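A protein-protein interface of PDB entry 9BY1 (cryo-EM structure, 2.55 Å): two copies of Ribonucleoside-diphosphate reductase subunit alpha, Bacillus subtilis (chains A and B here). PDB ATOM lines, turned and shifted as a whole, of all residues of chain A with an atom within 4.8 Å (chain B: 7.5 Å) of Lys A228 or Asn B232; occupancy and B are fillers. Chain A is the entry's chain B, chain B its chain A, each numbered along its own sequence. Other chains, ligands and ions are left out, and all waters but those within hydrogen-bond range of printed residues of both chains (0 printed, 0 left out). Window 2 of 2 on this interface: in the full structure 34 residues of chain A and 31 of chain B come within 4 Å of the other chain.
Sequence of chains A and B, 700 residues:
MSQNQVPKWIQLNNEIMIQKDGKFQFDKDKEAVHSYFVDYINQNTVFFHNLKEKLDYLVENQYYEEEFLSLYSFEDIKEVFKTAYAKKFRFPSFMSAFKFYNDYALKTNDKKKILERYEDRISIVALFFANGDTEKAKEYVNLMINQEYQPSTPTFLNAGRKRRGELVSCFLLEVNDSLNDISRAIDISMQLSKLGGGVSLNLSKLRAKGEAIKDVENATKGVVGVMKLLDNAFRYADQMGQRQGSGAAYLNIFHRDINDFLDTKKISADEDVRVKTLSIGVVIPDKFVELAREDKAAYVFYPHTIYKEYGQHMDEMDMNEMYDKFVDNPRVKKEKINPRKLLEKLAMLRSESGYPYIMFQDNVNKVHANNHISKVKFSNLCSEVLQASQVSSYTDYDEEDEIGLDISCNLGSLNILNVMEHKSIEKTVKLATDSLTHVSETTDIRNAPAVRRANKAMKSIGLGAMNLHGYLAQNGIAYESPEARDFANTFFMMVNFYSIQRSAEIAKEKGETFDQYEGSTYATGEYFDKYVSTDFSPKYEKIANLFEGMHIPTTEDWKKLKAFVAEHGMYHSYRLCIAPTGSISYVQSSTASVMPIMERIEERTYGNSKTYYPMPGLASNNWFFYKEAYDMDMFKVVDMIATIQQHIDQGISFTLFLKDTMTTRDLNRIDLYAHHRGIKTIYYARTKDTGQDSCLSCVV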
ATOM      1  N   VAL A 224     -16.983  -8.418  18.728  1.00  0.00           N
ATOM      2  CA  VAL A 224     -16.385  -7.737  19.872  1.00  0.00           C
ATOM      3  C   VAL A 224     -15.877  -6.346  19.497  1.00  0.00           C
ATOM      4  O   VAL A 224     -15.922  -5.425  20.320  1.00  0.00           O
ATOM      5  CB  VAL A 224     -15.271  -8.603  20.480  1.00  0.00           C
ATOM      6  CG1 VAL A 224     -14.733  -7.967  21.749  1.00  0.00           C
ATOM      7  CG2 VAL A 224     -15.793  -9.998  20.766  1.00  0.00           C
ATOM      8  N   GLY A 225     -15.391  -6.157  18.270  1.00  0.00           N
ATOM      9  CA  GLY A 225     -15.045  -4.813  17.834  1.00  0.00           C
ATOM     10  C   GLY A 225     -16.253  -3.898  17.785  1.00  0.00           C
ATOM     11  O   GLY A 225     -16.197  -2.746  18.232  1.00  0.00           O
ATOM     12  N   VAL A 226     -17.367  -4.403  17.251  1.00  0.00           N
ATOM     13  CA  VAL A 226     -18.615  -3.651  17.270  1.00  0.00           C
ATOM     14  C   VAL A 226     -19.080  -3.430  18.702  1.00  0.00           C
ATOM     15  O   VAL A 226     -19.656  -2.387  19.021  1.00  0.00           O
ATOM     16  CB  VAL A 226     -19.685  -4.374  16.431  1.00  0.00           C
ATOM     17  CG1 VAL A 226     -20.959  -3.549  16.362  1.00  0.00           C
ATOM     18  CG2 VAL A 226     -19.154  -4.658  15.040  1.00  0.00           C
ATOM     19  N   MET A 227     -18.840  -4.402  19.582  1.00  0.00           N
ATOM     20  CA  MET A 227     -19.189  -4.244  20.989  1.00  0.00           C
ATOM     21  C   MET A 227     -18.418  -3.095  21.624  1.00  0.00           C
ATOM     22  O   MET A 227     -18.987  -2.300  22.377  1.00  0.00           O
ATOM     23  CB  MET A 227     -18.914  -5.546  21.737  1.00  0.00           C
ATOM     24  CG  MET A 227     -20.036  -6.555  21.675  1.00  0.00           C
ATOM     25  SD  MET A 227     -19.746  -7.906  22.820  1.00  0.00           S
ATOM     26  CE  MET A 227     -20.444  -7.213  24.305  1.00  0.00           C
ATOM     27  N   LYS A 228     -17.119  -3.000  21.340  1.00  0.00           N
ATOM     28  CA  LYS A 228     -16.321  -1.887  21.849  1.00  0.00           C
ATOM     29  C   LYS A 228     -16.800  -0.558  21.280  1.00  0.00           C
ATOM     30  O   LYS A 228     -16.892   0.444  22.004  1.00  0.00           O
ATOM     31  CB  LYS A 228     -14.846  -2.100  21.516  1.00  0.00           C
ATOM     32  CG  LYS A 228     -14.245  -3.361  22.096  1.00  0.00           C
ATOM     33  CD  LYS A 228     -12.732  -3.279  22.096  1.00  0.00           C
ATOM     34  CE  LYS A 228     -12.143  -3.912  20.844  1.00  0.00           C
ATOM     35  NZ  LYS A 228     -12.095  -5.396  20.942  1.00  0.00           N
ATOM     36  N   LEU A 229     -17.100  -0.530  19.978  1.00  0.00           N
ATOM     37  CA  LEU A 229     -17.619   0.687  19.364  1.00  0.00           C
ATOM     38  C   LEU A 229     -18.912   1.128  20.034  1.00  0.00           C
ATOM     39  O   LEU A 229     -19.092   2.308  20.350  1.00  0.00           O
ATOM     40  CB  LEU A 229     -17.849   0.470  17.870  1.00  0.00           C
ATOM     41  CG  LEU A 229     -16.657   0.516  16.920  1.00  0.00           C
ATOM     42  CD1 LEU A 229     -17.055  -0.097  15.593  1.00  0.00           C
ATOM     43  CD2 LEU A 229     -16.183   1.942  16.730  1.00  0.00           C
ATOM     44  N   LEU A 230     -19.822   0.181  20.271  1.00  0.00           N
ATOM     45  CA  LEU A 230     -21.101   0.505  20.890  1.00  0.00           C
ATOM     46  C   LEU A 230     -20.925   0.918  22.345  1.00  0.00           C
ATOM     47  O   LEU A 230     -21.634   1.803  22.830  1.00  0.00           O
ATOM     48  CB  LEU A 230     -22.051  -0.685  20.781  1.00  0.00           C
ATOM     49  CG  LEU A 230     -22.537  -1.026  19.374  1.00  0.00           C
ATOM     50  CD1 LEU A 230     -23.297  -2.340  19.381  1.00  0.00           C
ATOM     51  CD2 LEU A 230     -23.396   0.097  18.814  1.00  0.00           C
ATOM     52  N   ASP A 231     -19.996   0.282  23.059  1.00  0.00           N
ATOM     53  CA  ASP A 231     -19.746   0.659  24.444  1.00  0.00           C
ATOM     54  C   ASP A 231     -19.241   2.091  24.537  1.00  0.00           C
ATOM     55  O   ASP A 231     -19.705   2.869  25.378  1.00  0.00           O
ATOM     56  CB  ASP A 231     -18.749  -0.309  25.078  1.00  0.00           C
ATOM     57  CG  ASP A 231     -18.591  -0.089  26.568  1.00  0.00           C
ATOM     58  OD1 ASP A 231     -19.494  -0.492  27.328  1.00  0.00           O
ATOM     59  OD2 ASP A 231     -17.563   0.487  26.981  1.00  0.00           O
ATOM     60  N   ASN A 232     -18.304   2.465  23.665  1.00  0.00           N
ATOM     61  CA  ASN A 232     -17.831   3.847  23.658  1.00  0.00           C
ATOM     62  C   ASN A 232     -18.911   4.810  23.180  1.00  0.00           C
ATOM     63  O   ASN A 232     -18.989   5.947  23.660  1.00  0.00           O
ATOM     64  CB  ASN A 232     -16.571   3.963  22.807  1.00  0.00           C
ATOM     65  CG  ASN A 232     -15.314   3.802  23.626  1.00  0.00           C
ATOM     66  OD1 ASN A 232     -15.193   4.370  24.710  1.00  0.00           O
ATOM     67  ND2 ASN A 232     -14.393   2.993  23.141  1.00  0.00           N
ATOM     68  N   ASP A 272      -8.880  -4.378  26.378  1.00  0.00           N
ATOM     69  CA  ASP A 272      -9.206  -4.311  24.960  1.00  0.00           C
ATOM     70  C   ASP A 272     -10.324  -5.269  24.571  1.00  0.00           C
ATOM     71  O   ASP A 272     -10.701  -5.318  23.396  1.00  0.00           O
ATOM     72  CB  ASP A 272      -7.958  -4.583  24.109  1.00  0.00           C
ATOM     73  CG  ASP A 272      -7.568  -6.050  24.088  1.00  0.00           C
ATOM     74  OD1 ASP A 272      -7.828  -6.758  25.081  1.00  0.00           O
ATOM     75  OD2 ASP A 272      -6.996  -6.495  23.070  1.00  0.00           O
ATOM     76  N   VAL A 273     -10.846  -6.042  25.525  1.00  0.00           N
ATOM     77  CA  VAL A 273     -11.975  -6.931  25.300  1.00  0.00           C
ATOM     78  C   VAL A 273     -13.171  -6.553  26.163  1.00  0.00           C
ATOM     79  O   VAL A 273     -14.318  -6.605  25.703  1.00  0.00           O
ATOM     80  CB  VAL A 273     -11.578  -8.403  25.542  1.00  0.00           C
ATOM     81  CG1 VAL A 273     -12.770  -9.326  25.332  1.00  0.00           C
ATOM     82  CG2 VAL A 273     -10.423  -8.798  24.634  1.00  0.00           C
ATOM     83  N   VAL A 275     -16.159  -4.825  28.057  1.00  0.00           N
ATOM     84  CA  VAL A 275     -17.105  -3.733  27.859  1.00  0.00           C
ATOM     85  C   VAL A 275     -17.775  -3.447  29.196  1.00  0.00           C
ATOM     86  O   VAL A 275     -18.117  -4.373  29.940  1.00  0.00           O
ATOM     87  CB  VAL A 275     -18.145  -4.063  26.770  1.00  0.00           C
ATOM     88  CG1 VAL A 275     -17.490  -4.079  25.398  1.00  0.00           C
ATOM     89  CG2 VAL A 275     -18.817  -5.394  27.053  1.00  0.00           C
ATOM     90  N   ILE B 186     -17.484   9.920  12.497  1.00  0.00           N
ATOM     91  CA  ILE B 186     -17.042   8.566  12.831  1.00  0.00           C
ATOM     92  C   ILE B 186     -17.273   7.626  11.655  1.00  0.00           C
ATOM     93  O   ILE B 186     -16.399   6.826  11.292  1.00  0.00           O
ATOM     94  CB  ILE B 186     -17.759   8.068  14.099  1.00  0.00           C
ATOM     95  CG1 ILE B 186     -17.270   8.825  15.331  1.00  0.00           C
ATOM     96  CG2 ILE B 186     -17.556   6.571  14.280  1.00  0.00           C
ATOM     97  CD1 ILE B 186     -18.198   8.698  16.517  1.00  0.00           C
ATOM     98  N   MET B 190     -14.317   5.759   9.477  1.00  0.00           N
ATOM     99  CA  MET B 190     -14.232   4.315   9.284  1.00  0.00           C
ATOM    100  C   MET B 190     -14.273   3.944   7.805  1.00  0.00           C
ATOM    101  O   MET B 190     -13.557   3.035   7.372  1.00  0.00           O
ATOM    102  CB  MET B 190     -15.344   3.607  10.054  1.00  0.00           C
ATOM    103  CG  MET B 190     -15.054   3.460  11.537  1.00  0.00           C
ATOM    104  SD  MET B 190     -16.459   2.920  12.527  1.00  0.00           S
ATOM    105  CE  MET B 190     -17.813   3.235  11.405  1.00  0.00           C
ATOM    106  N   VAL B 226     -15.068  12.673  21.877  1.00  0.00           N
ATOM    107  CA  VAL B 226     -15.022  12.452  20.436  1.00  0.00           C
ATOM    108  C   VAL B 226     -13.691  11.839  20.038  1.00  0.00           C
ATOM    109  O   VAL B 226     -13.622  11.036  19.102  1.00  0.00           O
ATOM    110  CB  VAL B 226     -15.284  13.772  19.689  1.00  0.00           C
ATOM    111  CG1 VAL B 226     -15.433  13.522  18.195  1.00  0.00           C
ATOM    112  CG2 VAL B 226     -16.515  14.454  20.250  1.00  0.00           C
ATOM    113  N   MET B 227     -12.615  12.208  20.732  1.00  0.00           N
ATOM    114  CA  MET B 227     -11.308  11.622  20.466  1.00  0.00           C
ATOM    115  C   MET B 227     -11.307  10.127  20.755  1.00  0.00           C
ATOM    116  O   MET B 227     -10.752   9.342  19.983  1.00  0.00           O
ATOM    117  CB  MET B 227     -10.250  12.332  21.307  1.00  0.00           C
ATOM    118  CG  MET B 227      -9.725  13.611  20.694  1.00  0.00           C
ATOM    119  SD  MET B 227      -8.237  14.195  21.514  1.00  0.00           S
ATOM    120  CE  MET B 227      -7.024  13.096  20.808  1.00  0.00           C
ATOM    121  N   LYS B 228     -11.919   9.720  21.867  1.00  0.00           N
ATOM    122  CA  LYS B 228     -12.028   8.297  22.180  1.00  0.00           C
ATOM    123  C   LYS B 228     -12.893   7.571  21.157  1.00  0.00           C
ATOM    124  O   LYS B 228     -12.563   6.455  20.728  1.00  0.00           O
ATOM    125  CB  LYS B 228     -12.593   8.107  23.585  1.00  0.00           C
ATOM    126  CG  LYS B 228     -11.738   8.702  24.687  1.00  0.00           C
ATOM    127  CD  LYS B 228     -12.321   8.399  26.056  1.00  0.00           C
ATOM    128  CE  LYS B 228     -13.395   9.407  26.439  1.00  0.00           C
ATOM    129  NZ  LYS B 228     -12.906  10.386  27.445  1.00  0.00           N
ATOM    130  N   LEU B 229     -14.007   8.191  20.757  1.00  0.00           N
ATOM    131  CA  LEU B 229     -14.851   7.607  19.720  1.00  0.00           C
ATOM    132  C   LEU B 229     -14.065   7.390  18.433  1.00  0.00           C
ATOM    133  O   LEU B 229     -14.128   6.316  17.825  1.00  0.00           O
ATOM    134  CB  LEU B 229     -16.055   8.508  19.453  1.00  0.00           C
ATOM    135  CG  LEU B 229     -17.184   8.579  20.478  1.00  0.00           C
ATOM    136  CD1 LEU B 229     -18.058   9.773  20.161  1.00  0.00           C
ATOM    137  CD2 LEU B 229     -17.998   7.300  20.473  1.00  0.00           C
ATOM    138  N   LEU B 230     -13.312   8.405  18.008  1.00  0.00           N
ATOM    139  CA  LEU B 230     -12.532   8.304  16.780  1.00  0.00           C
ATOM    140  C   LEU B 230     -11.408   7.287  16.915  1.00  0.00           C
ATOM    141  O   LEU B 230     -11.096   6.569  15.960  1.00  0.00           O
ATOM    142  CB  LEU B 230     -11.971   9.674  16.403  1.00  0.00           C
ATOM    143  CG  LEU B 230     -12.982  10.679  15.855  1.00  0.00           C
ATOM    144  CD1 LEU B 230     -12.408  12.086  15.891  1.00  0.00           C
ATOM    145  CD2 LEU B 230     -13.400  10.295  14.447  1.00  0.00           C
ATOM    146  N   ASP B 231     -10.782   7.217  18.089  1.00  0.00           N
ATOM    147  CA  ASP B 231      -9.718   6.245  18.304  1.00  0.00           C
ATOM    148  C   ASP B 231     -10.243   4.823  18.180  1.00  0.00           C
ATOM    149  O   ASP B 231      -9.611   3.973  17.541  1.00  0.00           O
ATOM    150  CB  ASP B 231      -9.078   6.473  19.673  1.00  0.00           C
ATOM    151  CG  ASP B 231      -7.968   5.490  19.968  1.00  0.00           C
ATOM    152  OD1 ASP B 231      -6.919   5.554  19.295  1.00  0.00           O
ATOM    153  OD2 ASP B 231      -8.140   4.655  20.880  1.00  0.00           O
ATOM    154  N   ASN B 232     -11.412   4.547  18.760  1.00  0.00           N
ATOM    155  CA  ASN B 232     -11.985   3.213  18.608  1.00  0.00           C
ATOM    156  C   ASN B 232     -12.491   2.965  17.194  1.00  0.00           C
ATOM    157  O   ASN B 232     -12.442   1.827  16.714  1.00  0.00           O
ATOM    158  CB  ASN B 232     -13.103   2.993  19.621  1.00  0.00           C
ATOM    159  CG  ASN B 232     -12.578   2.536  20.957  1.00  0.00           C
ATOM    160  OD1 ASN B 232     -11.953   3.304  21.689  1.00  0.00           O
ATOM    161  ND2 ASN B 232     -12.823   1.273  21.286  1.00  0.00           N
ATOM    162  N   ALA B 233     -12.973   4.004  16.511  1.00  0.00           N
ATOM    163  CA  ALA B 233     -13.384   3.843  15.121  1.00  0.00           C
ATOM    164  C   ALA B 233     -12.197   3.486  14.237  1.00  0.00           C
ATOM    165  O   ALA B 233     -12.322   2.678  13.310  1.00  0.00           O
ATOM    166  CB  ALA B 233     -14.064   5.117  14.626  1.00  0.00           C
ATOM    167  N   PHE B 234     -11.037   4.086  14.504  1.00  0.00           N
ATOM    168  CA  PHE B 234      -9.836   3.776  13.740  1.00  0.00           C
ATOM    169  C   PHE B 234      -9.242   2.430  14.130  1.00  0.00           C
ATOM    170  O   PHE B 234      -8.653   1.750  13.284  1.00  0.00           O
ATOM    171  CB  PHE B 234      -8.804   4.889  13.911  1.00  0.00           C
ATOM    172  CG  PHE B 234      -9.104   6.114  13.098  1.00  0.00           C
ATOM    173  CD1 PHE B 234      -9.237   6.030  11.725  1.00  0.00           C
ATOM    174  CD2 PHE B 234      -9.271   7.343  13.705  1.00  0.00           C
ATOM    175  CE1 PHE B 234      -9.521   7.152  10.975  1.00  0.00           C
ATOM    176  CE2 PHE B 234      -9.559   8.467  12.963  1.00  0.00           C
ATOM    177  CZ  PHE B 234      -9.683   8.372  11.596  1.00  0.00           C
ATOM    178  N   ARG B 235      -9.372   2.031  15.397  1.00  0.00           N
ATOM    179  CA  ARG B 235      -8.979   0.678  15.776  1.00  0.00           C
ATOM    180  C   ARG B 235      -9.854  -0.369  15.105  1.00  0.00           C
ATOM    181  O   ARG B 235      -9.361  -1.440  14.736  1.00  0.00           O
ATOM    182  CB  ARG B 235      -9.028   0.507  17.291  1.00  0.00           C
ATOM    183  CG  ARG B 235      -7.663   0.344  17.924  1.00  0.00           C
ATOM    184  CD  ARG B 235      -7.749  -0.319  19.292  1.00  0.00           C
ATOM    185  NE  ARG B 235      -8.689   0.328  20.201  1.00  0.00           N
ATOM    186  CZ  ARG B 235      -8.618   1.591  20.603  1.00  0.00           C
ATOM    187  NH1 ARG B 235      -7.629   2.386  20.226  1.00  0.00           N
ATOM    188  NH2 ARG B 235      -9.550   2.063  21.424  1.00  0.00           N
ATOM    189  N   TYR B 236     -11.149  -0.090  14.951  1.00  0.00           N
ATOM    190  CA  TYR B 236     -12.034  -1.053  14.307  1.00  0.00           C
ATOM    191  C   TYR B 236     -11.714  -1.191  12.824  1.00  0.00           C
ATOM    192  O   TYR B 236     -11.586  -2.306  12.307  1.00  0.00           O
ATOM    193  CB  TYR B 236     -13.491  -0.642  14.503  1.00  0.00           C
ATOM    194  CG  TYR B 236     -14.467  -1.644  13.945  1.00  0.00           C
ATOM    195  CD1 TYR B 236     -14.673  -2.859  14.578  1.00  0.00           C
ATOM    196  CD2 TYR B 236     -15.173  -1.385  12.778  1.00  0.00           C
ATOM    197  CE1 TYR B 236     -15.555  -3.783  14.076  1.00  0.00           C
ATOM    198  CE2 TYR B 236     -16.062  -2.307  12.266  1.00  0.00           C
ATOM    199  CZ  TYR B 236     -16.248  -3.503  12.922  1.00  0.00           C
ATOM    200  OH  TYR B 236     -17.128  -4.432  12.429  1.00  0.00           O
ATOM    201  N   ALA B 237     -11.584  -0.066  12.120  1.00  0.00           N
ATOM    202  CA  ALA B 237     -11.282  -0.076  10.691  1.00  0.00           C
ATOM    203  C   ALA B 237      -9.766  -0.079  10.521  1.00  0.00           C
ATOM    204  O   ALA B 237      -9.122   0.955  10.327  1.00  0.00           O
ATOM    205  CB  ALA B 237     -11.934   1.110   9.993  1.00  0.00           C
ATOM    206  N   ARG B 274      -6.480   8.338  27.512  1.00  0.00           N
ATOM    207  CA  ARG B 274      -5.437   8.197  26.506  1.00  0.00           C
ATOM    208  C   ARG B 274      -5.982   7.604  25.212  1.00  0.00           C
ATOM    209  O   ARG B 274      -6.777   6.661  25.224  1.00  0.00           O
ATOM    210  CB  ARG B 274      -4.304   7.323  27.051  1.00  0.00           C
ATOM    211  CG  ARG B 274      -3.652   6.416  26.020  1.00  0.00           C
ATOM    212  CD  ARG B 274      -2.373   5.790  26.560  1.00  0.00           C
ATOM    213  NE  ARG B 274      -1.284   6.750  26.717  1.00  0.00           N
ATOM    214  CZ  ARG B 274      -0.746   7.466  25.737  1.00  0.00           C
ATOM    215  NH1 ARG B 274      -1.138   7.332  24.479  1.00  0.00           N
ATOM    216  NH2 ARG B 274       0.225   8.328  26.024  1.00  0.00           N
ATOM    217  N   VAL B 275      -5.548   8.174  24.089  1.00  0.00           N
ATOM    218  CA  VAL B 275      -5.826   7.647  22.760  1.00  0.00           C
ATOM    219  C   VAL B 275      -4.514   7.149  22.171  1.00  0.00           C
ATOM    220  O   VAL B 275      -3.468   7.791  22.330  1.00  0.00           O
ATOM    221  CB  VAL B 275      -6.481   8.700  21.846  1.00  0.00           C
ATOM    222  CG1 VAL B 275      -7.895   9.003  22.316  1.00  0.00           C
ATOM    223  CG2 VAL B 275      -5.651   9.969  21.810  1.00  0.00           C
ATOM    224  N   THR B 277      -4.270   5.196  18.757  1.00  0.00           N
ATOM    225  CA  THR B 277      -4.210   5.171  17.303  1.00  0.00           C
ATOM    226  C   THR B 277      -4.482   6.531  16.677  1.00  0.00           C
ATOM    227  O   THR B 277      -4.556   6.632  15.448  1.00  0.00           O
ATOM    228  CB  THR B 277      -5.197   4.142  16.750  1.00  0.00           C
ATOM    229  OG1 THR B 277      -6.475   4.760  16.557  1.00  0.00           O
ATOM    230  CG2 THR B 277      -5.342   2.987  17.717  1.00  0.00           C
ATOM    231  N   LEU B 278      -4.631   7.575  17.486  1.00  0.00           N
ATOM    232  CA  LEU B 278      -5.009   8.899  17.005  1.00  0.00           C
ATOM    233  C   LEU B 278      -3.854   9.862  17.241  1.00  0.00           C
ATOM    234  O   LEU B 278      -3.555  10.207  18.387  1.00  0.00           O
ATOM    235  CB  LEU B 278      -6.278   9.387  17.701  1.00  0.00           C
ATOM    236  CG  LEU B 278      -7.109  10.438  16.967  1.00  0.00           C
ATOM    237  CD1 LEU B 278      -7.829   9.825  15.782  1.00  0.00           C
ATOM    238  CD2 LEU B 278      -8.102  11.075  17.919  1.00  0.00           C
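The backbone carbonyl oxygen of Lys B228 sits close to the side-chain amide oxygen of Asn B232. The guanidinium group (NH2) of Arg B235 sits at hydrogen-bond distance from the side-chain amide oxygen (OD1) of Asn B232 (2.7 Å). The side-chain amino group (NZ) of Lys A228 lies within hydrogen-bond range of the backbone carbonyl oxygen (O) of Asp A272 (2.8 Å).
Val A224 touches none of the printed residues of chain B. Of chain B, only Asn B232 (3.9 Å) comes within 4 Å of Lys A228. Met B227 touches none of the printed residues of chain A. Of the printed residues of chain A, Leu B229 touches Asn A232 (3.6 Å). Asn B232 touches just these residues of chain A: Lys A228 (3.9 Å), Leu A229 (3.7 Å) and Asn A232 (2.9 Å). Of the printed residues of chain A, Ala B233 touches Leu A229 (3.7 Å). Printed residues of chain A within 4 Å of Tyr B236: Gly A225 (3.7 Å), Val A226 (3.3 Å) and Leu A229 (3.4 Å).
OD1 of Asn B232 is in hydrogen-bond range of ND2 of Asn A232, 2.9 Å away.
Among the printed residues, pairs that only touch across the chains: Val A226 with Tyr B236, Leu A229 with Tyr B236, Asn A232 with Leu B229, Gly A225 with Tyr B236, Leu A229 with Asn B232, Leu A229 with Ala B233 and Lys A228 with Asn B232.
Lys A228 touches Asn B232, but with the chains exchanged Asn A232 does not touch Lys B228 (4.6 Å). Leu A229 touches Asn B232, and with the chains exchanged Asn A232 touches Leu B229. Asn B232 touches its own counterpart, Asn A232.
Of the 12 printed residues of chain A, 5 touch a printed residue of chain B. Printed residues of chain B that touch a printed residue of chain A: Leu B229, Asn B232, Ala B233 and Tyr B236. Hydrophobic or aromatic side chains of chain B within 4 Å of the printed part of chain A: Leu B229 and Tyr B236. Among the printed residues, 8 pairs touch across the chains. Among the printed residues, no Asp or Glu carboxylate lies within 4 Å of a Lys or Arg side-chain nitrogen of the other chain.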
